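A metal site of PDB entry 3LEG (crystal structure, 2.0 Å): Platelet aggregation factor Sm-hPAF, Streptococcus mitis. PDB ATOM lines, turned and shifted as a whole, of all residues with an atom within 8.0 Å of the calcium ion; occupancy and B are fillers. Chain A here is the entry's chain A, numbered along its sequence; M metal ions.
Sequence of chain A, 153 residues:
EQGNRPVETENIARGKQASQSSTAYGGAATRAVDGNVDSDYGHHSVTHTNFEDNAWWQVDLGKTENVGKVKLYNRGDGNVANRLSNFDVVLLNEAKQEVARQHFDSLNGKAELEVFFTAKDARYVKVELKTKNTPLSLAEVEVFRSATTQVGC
The calcium ion is bound by the backbone carbonyl oxygen of Arg 31 (2.3 Å), the backbone carbonyl oxygen of Ala 139 (2.3 Å), the backbone carbonyl oxygen of Asn 36 (2.3 Å), the side-chain hydroxyl of Ser 45 (2.3 Å), the side-chain carboxylate of Asp 34 (2.4 Å), the side-chain carboxylate of Glu 140 (2.4 Å) and the backbone carbonyl oxygen of Ser 45 (2.4 Å).
The calcium ion has seven donor atoms within binding distance.
The guanidinium group (NE) of Arg 31 sits at hydrogen-bond distance from the backbone carbonyl oxygen (O) of His 44 (3.2 Å).
The backbone NH of Ala 139 sits at hydrogen-bond distance from the backbone carbonyl oxygen of Tyr 73, 2.9 Å away.
OE2 of Glu 140 sits at hydrogen-bond distance from N of Gly 35.
O of Glu 140 lies within hydrogen-bond range of N of Tyr 73.
The side-chain amide oxygen of Asn 36 sits at hydrogen-bond distance from the backbone NH of Asp 38 (3.0 Å).
Of the 22 residues printed, 6 come within 4 Å of the calcium ion.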
ATOM      1  N   ALA A  28      23.671  10.535  25.051  1.00  0.00           N
ATOM      2  CA  ALA A  28      22.491   9.748  25.475  1.00  0.00           C
ATOM      3  C   ALA A  28      21.215  10.189  24.767  1.00  0.00           C
ATOM      4  O   ALA A  28      20.939  11.383  24.667  1.00  0.00           O
ATOM      5  CB  ALA A  28      22.303   9.819  27.005  1.00  0.00           C
ATOM      6  N   ALA A  29      20.418   9.208  24.310  1.00  0.00           N
ATOM      7  CA  ALA A  29      19.105   9.473  23.692  1.00  0.00           C
ATOM      8  C   ALA A  29      18.192  10.368  24.547  1.00  0.00           C
ATOM      9  O   ALA A  29      17.449  11.174  23.996  1.00  0.00           O
ATOM     10  CB  ALA A  29      18.384   8.149  23.373  1.00  0.00           C
ATOM     11  N   THR A  30      18.268  10.234  25.872  1.00  0.00           N
ATOM     12  CA  THR A  30      17.423  11.000  26.765  1.00  0.00           C
ATOM     13  C   THR A  30      17.711  12.510  26.659  1.00  0.00           C
ATOM     14  O   THR A  30      16.899  13.311  27.128  1.00  0.00           O
ATOM     15  CB  THR A  30      17.564  10.545  28.227  1.00  0.00           C
ATOM     16  OG1 THR A  30      18.963  10.477  28.577  1.00  0.00           O
ATOM     17  CG2 THR A  30      16.937   9.195  28.436  1.00  0.00           C
ATOM     18  N   ARG A  31      18.839  12.918  26.047  1.00  0.00           N
ATOM     19  CA  ARG A  31      19.189  14.369  25.946  1.00  0.00           C
ATOM     20  C   ARG A  31      18.241  15.089  25.016  1.00  0.00           C
ATOM     21  O   ARG A  31      18.083  16.310  25.102  1.00  0.00           O
ATOM     22  CB  ARG A  31      20.640  14.591  25.484  1.00  0.00           C
ATOM     23  CG  ARG A  31      21.681  14.200  26.532  1.00  0.00           C
ATOM     24  CD  ARG A  31      23.072  14.156  25.952  1.00  0.00           C
ATOM     25  NE  ARG A  31      24.076  13.814  26.965  1.00  0.00           N
ATOM     26  CZ  ARG A  31      25.383  14.031  26.816  1.00  0.00           C
ATOM     27  NH1 ARG A  31      26.220  13.733  27.809  1.00  0.00           N
ATOM     28  NH2 ARG A  31      25.866  14.530  25.663  1.00  0.00           N
ATOM     29  N   ALA A  32      17.587  14.348  24.132  1.00  0.00           N
ATOM     30  CA  ALA A  32      16.596  14.984  23.286  1.00  0.00           C
ATOM     31  C   ALA A  32      15.228  15.263  23.988  1.00  0.00           C
ATOM     32  O   ALA A  32      14.382  15.974  23.434  1.00  0.00           O
ATOM     33  CB  ALA A  32      16.403  14.168  21.977  1.00  0.00           C
ATOM     34  N   VAL A  33      15.003  14.702  25.178  1.00  0.00           N
ATOM     35  CA  VAL A  33      13.742  14.948  25.903  1.00  0.00           C
ATOM     36  C   VAL A  33      13.962  15.452  27.334  1.00  0.00           C
ATOM     37  O   VAL A  33      13.125  15.215  28.196  1.00  0.00           O
ATOM     38  CB  VAL A  33      12.797  13.707  25.886  1.00  0.00           C
ATOM     39  CG1 VAL A  33      12.272  13.451  24.399  1.00  0.00           C
ATOM     40  CG2 VAL A  33      13.516  12.479  26.465  1.00  0.00           C
ATOM     41  N   ASP A  34      15.094  16.143  27.557  1.00  0.00           N
ATOM     42  CA  ASP A  34      15.467  16.588  28.882  1.00  0.00           C
ATOM     43  C   ASP A  34      14.999  17.996  29.182  1.00  0.00           C
ATOM     44  O   ASP A  34      15.336  18.530  30.213  1.00  0.00           O
ATOM     45  CB  ASP A  34      16.980  16.469  29.092  1.00  0.00           C
ATOM     46  CG  ASP A  34      17.814  17.436  28.207  1.00  0.00           C
ATOM     47  OD1 ASP A  34      17.317  18.108  27.245  1.00  0.00           O
ATOM     48  OD2 ASP A  34      19.046  17.428  28.456  1.00  0.00           O
ATOM     49  N   GLY A  35      14.207  18.577  28.301  1.00  0.00           N
ATOM     50  CA  GLY A  35      13.634  19.894  28.534  1.00  0.00           C
ATOM     51  C   GLY A  35      14.647  21.005  28.352  1.00  0.00           C
ATOM     52  O   GLY A  35      14.507  22.087  28.920  1.00  0.00           O
ATOM     53  N   ASN A  36      15.688  20.737  27.552  1.00  0.00           N
ATOM     54  CA  ASN A  36      16.704  21.766  27.322  1.00  0.00           C
ATOM     55  C   ASN A  36      17.030  21.798  25.850  1.00  0.00           C
ATOM     56  O   ASN A  36      17.584  20.853  25.340  1.00  0.00           O
ATOM     57  CB  ASN A  36      17.931  21.461  28.205  1.00  0.00           C
ATOM     58  CG  ASN A  36      19.052  22.526  28.080  1.00  0.00           C
ATOM     59  OD1 ASN A  36      18.985  23.456  27.290  1.00  0.00           O
ATOM     60  ND2 ASN A  36      20.112  22.321  28.842  1.00  0.00           N
ATOM     61  N   VAL A  37      16.708  22.891  25.156  1.00  0.00           N
ATOM     62  CA  VAL A  37      16.938  22.943  23.708  1.00  0.00           C
ATOM     63  C   VAL A  37      18.314  23.497  23.347  1.00  0.00           C
ATOM     64  O   VAL A  37      18.602  23.727  22.150  1.00  0.00           O
ATOM     65  CB  VAL A  37      15.866  23.798  22.987  1.00  0.00           C
ATOM     66  CG1 VAL A  37      14.456  23.310  23.329  1.00  0.00           C
ATOM     67  CG2 VAL A  37      16.042  25.308  23.313  1.00  0.00           C
ATOM     68  N   ASP A  38      19.154  23.766  24.345  1.00  0.00           N
ATOM     69  CA  ASP A  38      20.525  24.218  24.054  1.00  0.00           C
ATOM     70  C   ASP A  38      21.228  23.335  23.006  1.00  0.00           C
ATOM     71  O   ASP A  38      21.441  22.153  23.233  1.00  0.00           O
ATOM     72  CB  ASP A  38      21.369  24.145  25.340  1.00  0.00           C
ATOM     73  CG  ASP A  38      22.661  24.918  25.227  1.00  0.00           C
ATOM     74  OD1 ASP A  38      23.078  25.470  26.274  1.00  0.00           O
ATOM     75  OD2 ASP A  38      23.274  24.981  24.132  1.00  0.00           O
ATOM     76  N   SER A  39      21.604  23.913  21.885  1.00  0.00           N
ATOM     77  CA  SER A  39      22.064  23.103  20.770  1.00  0.00           C
ATOM     78  C   SER A  39      23.606  22.914  20.692  1.00  0.00           C
ATOM     79  O   SER A  39      24.115  22.297  19.753  1.00  0.00           O
ATOM     80  CB  SER A  39      21.521  23.697  19.462  1.00  0.00           C
ATOM     81  OG  SER A  39      22.137  24.954  19.237  1.00  0.00           O
ATOM     82  N   HIS A  43      27.464  21.401  25.813  1.00  0.00           N
ATOM     83  CA  HIS A  43      26.563  21.684  26.955  1.00  0.00           C
ATOM     84  C   HIS A  43      25.723  20.464  27.346  1.00  0.00           C
ATOM     85  O   HIS A  43      24.871  20.563  28.223  1.00  0.00           O
ATOM     86  CB  HIS A  43      25.689  22.943  26.704  1.00  0.00           C
ATOM     87  CG  HIS A  43      26.491  24.187  26.437  1.00  0.00           C
ATOM     88  ND1 HIS A  43      25.934  25.359  25.999  1.00  0.00           N
ATOM     89  CD2 HIS A  43      27.830  24.427  26.562  1.00  0.00           C
ATOM     90  CE1 HIS A  43      26.888  26.276  25.850  1.00  0.00           C
ATOM     91  NE2 HIS A  43      28.050  25.732  26.196  1.00  0.00           N
ATOM     92  N   HIS A  44      26.013  19.318  26.683  1.00  0.00           N
ATOM     93  CA  HIS A  44      25.550  17.988  27.104  1.00  0.00           C
ATOM     94  C   HIS A  44      24.035  17.764  26.985  1.00  0.00           C
ATOM     95  O   HIS A  44      23.473  16.899  27.697  1.00  0.00           O
ATOM     96  CB  HIS A  44      25.977  17.723  28.573  1.00  0.00           C
ATOM     97  CG  HIS A  44      27.456  17.885  28.815  1.00  0.00           C
ATOM     98  ND1 HIS A  44      28.416  17.248  28.045  1.00  0.00           N
ATOM     99  CD2 HIS A  44      28.132  18.579  29.764  1.00  0.00           C
ATOM    100  CE1 HIS A  44      29.612  17.534  28.527  1.00  0.00           C
ATOM    101  NE2 HIS A  44      29.473  18.350  29.560  1.00  0.00           N
ATOM    102  N   SER A  45      23.372  18.501  26.113  1.00  0.00           N
ATOM    103  CA  SER A  45      21.914  18.302  25.964  1.00  0.00           C
ATOM    104  C   SER A  45      21.480  17.924  24.542  1.00  0.00           C
ATOM    105  O   SER A  45      20.277  18.123  24.192  1.00  0.00           O
ATOM    106  CB  SER A  45      21.115  19.493  26.461  1.00  0.00           C
ATOM    107  OG  SER A  45      19.728  19.090  26.616  1.00  0.00           O
ATOM    108  N   VAL A  46      22.469  17.435  23.772  1.00  0.00           N
ATOM    109  CA  VAL A  46      22.337  16.986  22.377  1.00  0.00           C
ATOM    110  C   VAL A  46      22.753  15.514  22.259  1.00  0.00           C
ATOM    111  O   VAL A  46      23.788  15.076  22.816  1.00  0.00           O
ATOM    112  CB  VAL A  46      23.256  17.842  21.406  1.00  0.00           C
ATOM    113  CG1 VAL A  46      23.011  17.468  19.974  1.00  0.00           C
ATOM    114  CG2 VAL A  46      23.086  19.372  21.641  1.00  0.00           C
ATOM    115  N   THR A  47      21.972  14.727  21.527  1.00  0.00           N
ATOM    116  CA  THR A  47      22.204  13.299  21.385  1.00  0.00           C
ATOM    117  C   THR A  47      23.248  13.076  20.298  1.00  0.00           C
ATOM    118  O   THR A  47      23.649  14.030  19.615  1.00  0.00           O
ATOM    119  CB  THR A  47      20.903  12.581  20.944  1.00  0.00           C
ATOM    120  OG1 THR A  47      20.603  12.982  19.596  1.00  0.00           O
ATOM    121  CG2 THR A  47      19.716  12.969  21.834  1.00  0.00           C
ATOM    122  N   TYR A  73      14.773  20.188  17.300  1.00  0.00           N
ATOM    123  CA  TYR A  73      15.812  21.206  17.446  1.00  0.00           C
ATOM    124  C   TYR A  73      17.156  20.620  17.009  1.00  0.00           C
ATOM    125  O   TYR A  73      17.564  19.603  17.530  1.00  0.00           O
ATOM    126  CB  TYR A  73      15.864  21.697  18.879  1.00  0.00           C
ATOM    127  CG  TYR A  73      14.595  22.394  19.344  1.00  0.00           C
ATOM    128  CD1 TYR A  73      14.556  23.782  19.474  1.00  0.00           C
ATOM    129  CD2 TYR A  73      13.451  21.669  19.663  1.00  0.00           C
ATOM    130  CE1 TYR A  73      13.458  24.419  19.918  1.00  0.00           C
ATOM    131  CE2 TYR A  73      12.279  22.323  20.095  1.00  0.00           C
ATOM    132  CZ  TYR A  73      12.297  23.694  20.233  1.00  0.00           C
ATOM    133  OH  TYR A  73      11.195  24.362  20.716  1.00  0.00           O
ATOM    134  N   LEU A 138      20.309  15.273  17.953  1.00  0.00           N
ATOM    135  CA  LEU A 138      19.167  16.138  18.172  1.00  0.00           C
ATOM    136  C   LEU A 138      19.345  16.905  19.484  1.00  0.00           C
ATOM    137  O   LEU A 138      19.623  16.293  20.535  1.00  0.00           O
ATOM    138  CB  LEU A 138      17.874  15.290  18.231  1.00  0.00           C
ATOM    139  CG  LEU A 138      17.478  14.618  16.894  1.00  0.00           C
ATOM    140  CD1 LEU A 138      16.603  13.330  17.078  1.00  0.00           C
ATOM    141  CD2 LEU A 138      16.760  15.633  15.997  1.00  0.00           C
ATOM    142  N   ALA A 139      19.163  18.226  19.450  1.00  0.00           N
ATOM    143  CA  ALA A 139      19.218  19.002  20.690  1.00  0.00           C
ATOM    144  C   ALA A 139      17.975  18.729  21.522  1.00  0.00           C
ATOM    145  O   ALA A 139      18.028  18.731  22.754  1.00  0.00           O
ATOM    146  CB  ALA A 139      19.333  20.507  20.360  1.00  0.00           C
ATOM    147  N   GLU A 140      16.843  18.512  20.857  1.00  0.00           N
ATOM    148  CA  GLU A 140      15.569  18.302  21.548  1.00  0.00           C
ATOM    149  C   GLU A 140      14.519  17.893  20.534  1.00  0.00           C
ATOM    150  O   GLU A 140      14.560  18.325  19.390  1.00  0.00           O
ATOM    151  CB  GLU A 140      15.075  19.574  22.230  1.00  0.00           C
ATOM    152  CG  GLU A 140      13.958  19.352  23.287  1.00  0.00           C
ATOM    153  CD  GLU A 140      14.462  18.812  24.635  1.00  0.00           C
ATOM    154  OE1 GLU A 140      15.710  18.600  24.819  1.00  0.00           O
ATOM    155  OE2 GLU A 140      13.579  18.608  25.516  1.00  0.00           O
ATOM    156  N   VAL A 141      13.593  17.016  20.980  1.00  0.00           N
ATOM    157  CA  VAL A 141      12.366  16.708  20.258  1.00  0.00           C
ATOM    158  C   VAL A 141      11.170  16.978  21.185  1.00  0.00           C
ATOM    159  O   VAL A 141      11.084  16.441  22.305  1.00  0.00           O
ATOM    160  CB  VAL A 141      12.314  15.243  19.745  1.00  0.00           C
ATOM    161  CG1 VAL A 141      10.974  14.965  19.071  1.00  0.00           C
ATOM    162  CG2 VAL A 141      13.493  14.949  18.768  1.00  0.00           C
HETATM  163 CA    CA M   1      18.085  18.606  25.049  1.00  0.00          CA
